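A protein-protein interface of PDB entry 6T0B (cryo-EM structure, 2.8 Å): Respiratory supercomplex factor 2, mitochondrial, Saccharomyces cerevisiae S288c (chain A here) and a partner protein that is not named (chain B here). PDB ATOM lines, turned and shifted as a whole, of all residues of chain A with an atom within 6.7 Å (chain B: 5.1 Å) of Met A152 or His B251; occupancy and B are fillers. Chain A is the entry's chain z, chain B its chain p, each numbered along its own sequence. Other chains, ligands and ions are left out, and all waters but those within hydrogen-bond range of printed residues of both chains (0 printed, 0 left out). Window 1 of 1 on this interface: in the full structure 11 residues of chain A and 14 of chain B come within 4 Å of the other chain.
Of the printed residues of chain B, Gln A149 touches Thr B153 (3.3 Å). Met A152 touches four residues of chain B. Printed residues of chain B within 4 Å of Gln A155: Leu B146 (3.7 Å). His B251 touches just these residues of chain A: Val A148 (3.4 Å), Arg A151 (3.5 Å) and Met A152 (3.5 Å). The nearest residue of chain A that does not touch His B251 is Gln A149 (5.1 Å).
Of the 14 printed residues of chain B, 6 touch a printed residue of chain A. Hydrophobic or aromatic side chains of chain A within 4 Å of the printed part of chain B: Val A148, Met A152 and Phe A156. Among the printed residues, no Asp or Glu carboxylate lies within 4 Å of a Lys or Arg side-chain nitrogen of the other chain.
Among the printed residues, merely in contact across the chains: Val A148 with Thr B153, Val A148 with Ile B248, Val A148 with His B251, Gln A149 with Thr B153, Arg A151 with Ile B248, Arg A151 with His B251, Met A152 with Leu B146, Met A152 with Gly B149, Met A152 with Ala B150, Met A152 with His B251, Gln A155 with Leu B146 and Phe A156 with Leu B146.
NE of Arg A151 lies within hydrogen-bond range of O of Ile A147, at 3.2 Å. The backbone carbonyl oxygen of Gly B149 lies within hydrogen-bond range of the side-chain hydroxyl of Thr B153, at 2.7 Å.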
ATOM      1  N   LEU A 128      -5.444 -23.298 -26.954  1.00  0.00           N
ATOM      2  CA  LEU A 128      -5.796 -21.964 -26.475  1.00  0.00           C
ATOM      3  C   LEU A 128      -5.048 -20.911 -27.272  1.00  0.00           C
ATOM      4  O   LEU A 128      -5.616 -19.860 -27.594  1.00  0.00           O
ATOM      5  CB  LEU A 128      -5.599 -21.812 -24.967  1.00  0.00           C
ATOM      6  CG  LEU A 128      -6.340 -20.582 -24.405  1.00  0.00           C
ATOM      7  CD1 LEU A 128      -6.939 -20.927 -23.049  1.00  0.00           C
ATOM      8  CD2 LEU A 128      -5.461 -19.316 -24.283  1.00  0.00           C
ATOM      9  N   SER A 131      -7.176 -20.935 -30.553  1.00  0.00           N
ATOM     10  CA  SER A 131      -8.411 -20.180 -30.612  1.00  0.00           C
ATOM     11  C   SER A 131      -8.210 -18.718 -30.260  1.00  0.00           C
ATOM     12  O   SER A 131      -9.065 -17.907 -30.615  1.00  0.00           O
ATOM     13  CB  SER A 131      -9.499 -20.782 -29.732  1.00  0.00           C
ATOM     14  OG  SER A 131     -10.644 -19.953 -29.785  1.00  0.00           O
ATOM     15  N   ILE A 147     -10.526 -13.293 -25.225  1.00  0.00           N
ATOM     16  CA  ILE A 147      -9.984 -14.280 -24.278  1.00  0.00           C
ATOM     17  C   ILE A 147     -11.095 -15.200 -23.755  1.00  0.00           C
ATOM     18  O   ILE A 147     -10.885 -16.415 -23.578  1.00  0.00           O
ATOM     19  CB  ILE A 147      -9.233 -13.558 -23.135  1.00  0.00           C
ATOM     20  CG1 ILE A 147      -7.959 -12.887 -23.659  1.00  0.00           C
ATOM     21  CG2 ILE A 147      -8.878 -14.496 -21.989  1.00  0.00           C
ATOM     22  CD1 ILE A 147      -6.759 -13.810 -23.806  1.00  0.00           C
ATOM     23  N   VAL A 148     -12.300 -14.629 -23.554  1.00  0.00           N
ATOM     24  CA  VAL A 148     -13.519 -15.368 -23.188  1.00  0.00           C
ATOM     25  C   VAL A 148     -13.765 -16.521 -24.152  1.00  0.00           C
ATOM     26  O   VAL A 148     -13.754 -17.698 -23.759  1.00  0.00           O
ATOM     27  CB  VAL A 148     -14.727 -14.404 -23.121  1.00  0.00           C
ATOM     28  CG1 VAL A 148     -16.077 -15.075 -23.205  1.00  0.00           C
ATOM     29  CG2 VAL A 148     -14.668 -13.575 -21.879  1.00  0.00           C
ATOM     30  N   GLN A 149     -13.918 -16.214 -25.438  1.00  0.00           N
ATOM     31  CA  GLN A 149     -14.313 -17.286 -26.333  1.00  0.00           C
ATOM     32  C   GLN A 149     -13.145 -18.166 -26.760  1.00  0.00           C
ATOM     33  O   GLN A 149     -13.378 -19.321 -27.143  1.00  0.00           O
ATOM     34  CB  GLN A 149     -15.057 -16.695 -27.514  1.00  0.00           C
ATOM     35  CG  GLN A 149     -16.427 -16.221 -27.078  1.00  0.00           C
ATOM     36  CD  GLN A 149     -17.243 -15.666 -28.203  1.00  0.00           C
ATOM     37  OE1 GLN A 149     -18.400 -15.298 -28.017  1.00  0.00           O
ATOM     38  NE2 GLN A 149     -16.661 -15.627 -29.395  1.00  0.00           N
ATOM     39  N   ALA A 150     -11.898 -17.690 -26.629  1.00  0.00           N
ATOM     40  CA  ALA A 150     -10.747 -18.566 -26.852  1.00  0.00           C
ATOM     41  C   ALA A 150     -10.660 -19.653 -25.780  1.00  0.00           C
ATOM     42  O   ALA A 150     -10.431 -20.839 -26.092  1.00  0.00           O
ATOM     43  CB  ALA A 150      -9.461 -17.740 -26.891  1.00  0.00           C
ATOM     44  N   ARG A 151     -10.844 -19.255 -24.508  1.00  0.00           N
ATOM     45  CA  ARG A 151     -10.921 -20.219 -23.412  1.00  0.00           C
ATOM     46  C   ARG A 151     -12.049 -21.218 -23.636  1.00  0.00           C
ATOM     47  O   ARG A 151     -11.849 -22.430 -23.454  1.00  0.00           O
ATOM     48  CB  ARG A 151     -11.117 -19.493 -22.078  1.00  0.00           C
ATOM     49  CG  ARG A 151      -9.856 -18.845 -21.519  1.00  0.00           C
ATOM     50  CD  ARG A 151     -10.125 -18.090 -20.218  1.00  0.00           C
ATOM     51  NE  ARG A 151     -11.032 -16.956 -20.395  1.00  0.00           N
ATOM     52  CZ  ARG A 151     -11.040 -15.873 -19.621  1.00  0.00           C
ATOM     53  NH1 ARG A 151     -10.179 -15.764 -18.620  1.00  0.00           N
ATOM     54  NH2 ARG A 151     -11.899 -14.891 -19.858  1.00  0.00           N
ATOM     55  N   MET A 152     -13.212 -20.725 -24.095  1.00  0.00           N
ATOM     56  CA  MET A 152     -14.368 -21.584 -24.373  1.00  0.00           C
ATOM     57  C   MET A 152     -14.045 -22.674 -25.393  1.00  0.00           C
ATOM     58  O   MET A 152     -14.223 -23.876 -25.121  1.00  0.00           O
ATOM     59  CB  MET A 152     -15.537 -20.735 -24.877  1.00  0.00           C
ATOM     60  CG  MET A 152     -16.142 -19.836 -23.836  1.00  0.00           C
ATOM     61  SD  MET A 152     -16.768 -20.793 -22.460  1.00  0.00           S
ATOM     62  CE  MET A 152     -18.119 -21.614 -23.283  1.00  0.00           C
ATOM     63  N   TYR A 153     -13.525 -22.260 -26.554  1.00  0.00           N
ATOM     64  CA  TYR A 153     -13.293 -23.176 -27.668  1.00  0.00           C
ATOM     65  C   TYR A 153     -12.253 -24.232 -27.321  1.00  0.00           C
ATOM     66  O   TYR A 153     -12.515 -25.442 -27.460  1.00  0.00           O
ATOM     67  CB  TYR A 153     -12.855 -22.388 -28.902  1.00  0.00           C
ATOM     68  CG  TYR A 153     -13.992 -21.713 -29.641  1.00  0.00           C
ATOM     69  CD1 TYR A 153     -15.270 -22.249 -29.614  1.00  0.00           C
ATOM     70  CD2 TYR A 153     -13.786 -20.542 -30.368  1.00  0.00           C
ATOM     71  CE1 TYR A 153     -16.315 -21.644 -30.286  1.00  0.00           C
ATOM     72  CE2 TYR A 153     -14.829 -19.929 -31.045  1.00  0.00           C
ATOM     73  CZ  TYR A 153     -16.090 -20.486 -30.998  1.00  0.00           C
ATOM     74  OH  TYR A 153     -17.131 -19.884 -31.666  1.00  0.00           O
ATOM     75  N   ALA A 154     -11.079 -23.787 -26.838  1.00  0.00           N
ATOM     76  CA  ALA A 154     -10.006 -24.719 -26.497  1.00  0.00           C
ATOM     77  C   ALA A 154     -10.418 -25.699 -25.416  1.00  0.00           C
ATOM     78  O   ALA A 154     -10.099 -26.904 -25.504  1.00  0.00           O
ATOM     79  CB  ALA A 154      -8.777 -23.962 -26.027  1.00  0.00           C
ATOM     80  N   GLN A 155     -11.168 -25.208 -24.414  1.00  0.00           N
ATOM     81  CA  GLN A 155     -11.589 -26.051 -23.318  1.00  0.00           C
ATOM     82  C   GLN A 155     -12.477 -27.174 -23.810  1.00  0.00           C
ATOM     83  O   GLN A 155     -12.061 -28.324 -23.644  1.00  0.00           O
ATOM     84  CB  GLN A 155     -12.293 -25.249 -22.237  1.00  0.00           C
ATOM     85  CG  GLN A 155     -12.581 -26.102 -21.027  1.00  0.00           C
ATOM     86  CD  GLN A 155     -11.322 -26.755 -20.475  1.00  0.00           C
ATOM     87  OE1 GLN A 155     -11.065 -27.941 -20.701  1.00  0.00           O
ATOM     88  NE2 GLN A 155     -10.544 -25.989 -19.726  1.00  0.00           N
ATOM     89  N   PHE A 156     -13.593 -26.882 -24.513  1.00  0.00           N
ATOM     90  CA  PHE A 156     -14.467 -28.014 -24.836  1.00  0.00           C
ATOM     91  C   PHE A 156     -13.882 -28.936 -25.902  1.00  0.00           C
ATOM     92  O   PHE A 156     -14.202 -30.129 -25.868  1.00  0.00           O
ATOM     93  CB  PHE A 156     -15.932 -27.609 -25.178  1.00  0.00           C
ATOM     94  CG  PHE A 156     -16.147 -26.798 -26.448  1.00  0.00           C
ATOM     95  CD1 PHE A 156     -16.121 -27.380 -27.712  1.00  0.00           C
ATOM     96  CD2 PHE A 156     -16.531 -25.473 -26.352  1.00  0.00           C
ATOM     97  CE1 PHE A 156     -16.350 -26.624 -28.845  1.00  0.00           C
ATOM     98  CE2 PHE A 156     -16.758 -24.710 -27.477  1.00  0.00           C
ATOM     99  CZ  PHE A 156     -16.679 -25.290 -28.723  1.00  0.00           C
ATOM    100  N   ILE A 157     -12.949 -28.463 -26.745  1.00  0.00           N
ATOM    101  CA  ILE A 157     -12.306 -29.381 -27.696  1.00  0.00           C
ATOM    102  C   ILE A 157     -11.454 -30.424 -26.971  1.00  0.00           C
ATOM    103  O   ILE A 157     -11.619 -31.642 -27.172  1.00  0.00           O
ATOM    104  CB  ILE A 157     -11.470 -28.601 -28.728  1.00  0.00           C
ATOM    105  CG1 ILE A 157     -12.360 -27.737 -29.620  1.00  0.00           C
ATOM    106  CG2 ILE A 157     -10.601 -29.533 -29.564  1.00  0.00           C
ATOM    107  CD1 ILE A 157     -13.423 -28.505 -30.358  1.00  0.00           C
ATOM    108  N   LEU B 146     -19.114 -25.556 -18.181  1.00  0.00           N
ATOM    109  CA  LEU B 146     -18.788 -25.032 -19.505  1.00  0.00           C
ATOM    110  C   LEU B 146     -20.043 -24.500 -20.193  1.00  0.00           C
ATOM    111  O   LEU B 146     -19.958 -23.622 -21.058  1.00  0.00           O
ATOM    112  CB  LEU B 146     -18.090 -26.103 -20.336  1.00  0.00           C
ATOM    113  CG  LEU B 146     -17.111 -25.634 -21.416  1.00  0.00           C
ATOM    114  CD1 LEU B 146     -16.143 -26.758 -21.632  1.00  0.00           C
ATOM    115  CD2 LEU B 146     -17.764 -25.275 -22.746  1.00  0.00           C
ATOM    116  N   GLY B 149     -20.358 -20.719 -19.193  1.00  0.00           N
ATOM    117  CA  GLY B 149     -19.600 -19.766 -19.990  1.00  0.00           C
ATOM    118  C   GLY B 149     -20.325 -19.368 -21.261  1.00  0.00           C
ATOM    119  O   GLY B 149     -20.366 -18.186 -21.621  1.00  0.00           O
ATOM    120  N   ALA B 150     -20.955 -20.340 -21.923  1.00  0.00           N
ATOM    121  CA  ALA B 150     -21.734 -20.048 -23.121  1.00  0.00           C
ATOM    122  C   ALA B 150     -22.972 -19.230 -22.786  1.00  0.00           C
ATOM    123  O   ALA B 150     -23.313 -18.290 -23.514  1.00  0.00           O
ATOM    124  CB  ALA B 150     -22.126 -21.346 -23.826  1.00  0.00           C
ATOM    125  N   VAL B 152     -23.347 -17.146 -20.161  1.00  0.00           N
ATOM    126  CA  VAL B 152     -23.011 -15.763 -19.810  1.00  0.00           C
ATOM    127  C   VAL B 152     -22.514 -14.999 -21.019  1.00  0.00           C
ATOM    128  O   VAL B 152     -22.680 -13.778 -21.082  1.00  0.00           O
ATOM    129  CB  VAL B 152     -21.978 -15.609 -18.673  1.00  0.00           C
ATOM    130  CG1 VAL B 152     -22.534 -16.031 -17.376  1.00  0.00           C
ATOM    131  CG2 VAL B 152     -20.634 -16.280 -18.978  1.00  0.00           C
ATOM    132  N   THR B 153     -21.894 -15.672 -21.989  1.00  0.00           N
ATOM    133  CA  THR B 153     -21.453 -14.927 -23.157  1.00  0.00           C
ATOM    134  C   THR B 153     -22.638 -14.542 -24.029  1.00  0.00           C
ATOM    135  O   THR B 153     -22.701 -13.414 -24.528  1.00  0.00           O
ATOM    136  CB  THR B 153     -20.420 -15.737 -23.930  1.00  0.00           C
ATOM    137  OG1 THR B 153     -19.371 -16.115 -23.035  1.00  0.00           O
ATOM    138  CG2 THR B 153     -19.825 -14.910 -25.040  1.00  0.00           C
ATOM    139  N   ILE B 247     -18.378 -11.748 -15.512  1.00  0.00           N
ATOM    140  CA  ILE B 247     -18.198 -12.701 -16.604  1.00  0.00           C
ATOM    141  C   ILE B 247     -16.742 -12.950 -16.950  1.00  0.00           C
ATOM    142  O   ILE B 247     -16.465 -13.813 -17.787  1.00  0.00           O
ATOM    143  CB  ILE B 247     -18.891 -12.297 -17.913  1.00  0.00           C
ATOM    144  CG1 ILE B 247     -18.257 -11.029 -18.458  1.00  0.00           C
ATOM    145  CG2 ILE B 247     -20.379 -12.137 -17.689  1.00  0.00           C
ATOM    146  CD1 ILE B 247     -18.632 -10.732 -19.847  1.00  0.00           C
ATOM    147  N   ILE B 248     -15.801 -12.213 -16.364  1.00  0.00           N
ATOM    148  CA  ILE B 248     -14.432 -12.725 -16.372  1.00  0.00           C
ATOM    149  C   ILE B 248     -14.232 -13.695 -15.200  1.00  0.00           C
ATOM    150  O   ILE B 248     -13.470 -14.676 -15.305  1.00  0.00           O
ATOM    151  CB  ILE B 248     -13.429 -11.557 -16.368  1.00  0.00           C
ATOM    152  CG1 ILE B 248     -13.621 -10.698 -17.618  1.00  0.00           C
ATOM    153  CG2 ILE B 248     -11.986 -12.037 -16.349  1.00  0.00           C
ATOM    154  CD1 ILE B 248     -13.450 -11.449 -18.920  1.00  0.00           C
ATOM    155  N   TYR B 249     -14.960 -13.471 -14.104  1.00  0.00           N
ATOM    156  CA  TYR B 249     -14.831 -14.322 -12.927  1.00  0.00           C
ATOM    157  C   TYR B 249     -15.359 -15.733 -13.179  1.00  0.00           C
ATOM    158  O   TYR B 249     -14.768 -16.707 -12.693  1.00  0.00           O
ATOM    159  CB  TYR B 249     -15.543 -13.649 -11.764  1.00  0.00           C
ATOM    160  CG  TYR B 249     -15.440 -14.313 -10.426  1.00  0.00           C
ATOM    161  CD1 TYR B 249     -14.236 -14.404  -9.750  1.00  0.00           C
ATOM    162  CD2 TYR B 249     -16.572 -14.775  -9.802  1.00  0.00           C
ATOM    163  CE1 TYR B 249     -14.170 -14.986  -8.500  1.00  0.00           C
ATOM    164  CE2 TYR B 249     -16.520 -15.349  -8.565  1.00  0.00           C
ATOM    165  CZ  TYR B 249     -15.323 -15.449  -7.914  1.00  0.00           C
ATOM    166  OH  TYR B 249     -15.300 -16.048  -6.679  1.00  0.00           O
ATOM    167  N   THR B 250     -16.449 -15.864 -13.954  1.00  0.00           N
ATOM    168  CA  THR B 250     -16.962 -17.192 -14.322  1.00  0.00           C
ATOM    169  C   THR B 250     -15.943 -17.991 -15.119  1.00  0.00           C
ATOM    170  O   THR B 250     -15.744 -19.189 -14.870  1.00  0.00           O
ATOM    171  CB  THR B 250     -18.242 -17.106 -15.154  1.00  0.00           C
ATOM    172  OG1 THR B 250     -17.933 -16.630 -16.471  1.00  0.00           O
ATOM    173  CG2 THR B 250     -19.302 -16.258 -14.513  1.00  0.00           C
ATOM    174  N   HIS B 251     -15.269 -17.338 -16.056  1.00  0.00           N
ATOM    175  CA  HIS B 251     -14.309 -18.038 -16.886  1.00  0.00           C
ATOM    176  C   HIS B 251     -13.070 -18.443 -16.113  1.00  0.00           C
ATOM    177  O   HIS B 251     -12.579 -19.568 -16.296  1.00  0.00           O
ATOM    178  CB  HIS B 251     -13.940 -17.174 -18.073  1.00  0.00           C
ATOM    179  CG  HIS B 251     -14.993 -17.165 -19.122  1.00  0.00           C
ATOM    180  ND1 HIS B 251     -14.876 -17.869 -20.297  1.00  0.00           N
ATOM    181  CD2 HIS B 251     -16.207 -16.574 -19.154  1.00  0.00           C
ATOM    182  CE1 HIS B 251     -15.970 -17.701 -21.015  1.00  0.00           C
ATOM    183  NE2 HIS B 251     -16.789 -16.908 -20.350  1.00  0.00           N
ATOM    184  N   VAL B 252     -12.569 -17.573 -15.234  1.00  0.00           N
ATOM    185  CA  VAL B 252     -11.378 -17.971 -14.495  1.00  0.00           C
ATOM    186  C   VAL B 252     -11.716 -19.047 -13.461  1.00  0.00           C
ATOM    187  O   VAL B 252     -10.922 -19.981 -13.246  1.00  0.00           O
ATOM    188  CB  VAL B 252     -10.686 -16.736 -13.878  1.00  0.00           C
ATOM    189  CG1 VAL B 252     -11.547 -16.019 -12.846  1.00  0.00           C
ATOM    190  CG2 VAL B 252      -9.324 -17.104 -13.303  1.00  0.00           C
ATOM    191  N   LEU B 253     -12.934 -19.031 -12.920  1.00  0.00           N
ATOM    192  CA  LEU B 253     -13.307 -20.079 -11.997  1.00  0.00           C
ATOM    193  C   LEU B 253     -13.731 -21.365 -12.675  1.00  0.00           C
ATOM    194  O   LEU B 253     -13.893 -22.371 -11.979  1.00  0.00           O
ATOM    195  CB  LEU B 253     -14.438 -19.634 -11.088  1.00  0.00           C
ATOM    196  CG  LEU B 253     -14.083 -19.065  -9.724  1.00  0.00           C
ATOM    197  CD1 LEU B 253     -15.363 -18.722  -9.088  1.00  0.00           C
ATOM    198  CD2 LEU B 253     -13.374 -20.083  -8.892  1.00  0.00           C
ATOM    199  N   ASP B 254     -13.959 -21.375 -13.983  1.00  0.00           N
ATOM    200  CA  ASP B 254     -14.080 -22.694 -14.588  1.00  0.00           C
ATOM    201  C   ASP B 254     -12.751 -23.228 -15.089  1.00  0.00           C
ATOM    202  O   ASP B 254     -12.588 -24.443 -15.158  1.00  0.00           O
ATOM    203  CB  ASP B 254     -15.145 -22.734 -15.690  1.00  0.00           C
ATOM    204  CG  ASP B 254     -14.838 -21.849 -16.886  1.00  0.00           C
ATOM    205  OD1 ASP B 254     -13.810 -22.035 -17.572  1.00  0.00           O
ATOM    206  OD2 ASP B 254     -15.688 -20.986 -17.183  1.00  0.00           O
ATOM    207  N   VAL B 255     -11.797 -22.369 -15.453  1.00  0.00           N
ATOM    208  CA  VAL B 255     -10.493 -22.895 -15.854  1.00  0.00           C
ATOM    209  C   VAL B 255      -9.751 -23.489 -14.652  1.00  0.00           C
ATOM    210  O   VAL B 255      -9.108 -24.546 -14.766  1.00  0.00           O
ATOM    211  CB  VAL B 255      -9.682 -21.812 -16.587  1.00  0.00           C
ATOM    212  CG1 VAL B 255      -8.308 -22.324 -16.973  1.00  0.00           C
ATOM    213  CG2 VAL B 255     -10.421 -21.414 -17.837  1.00  0.00           C
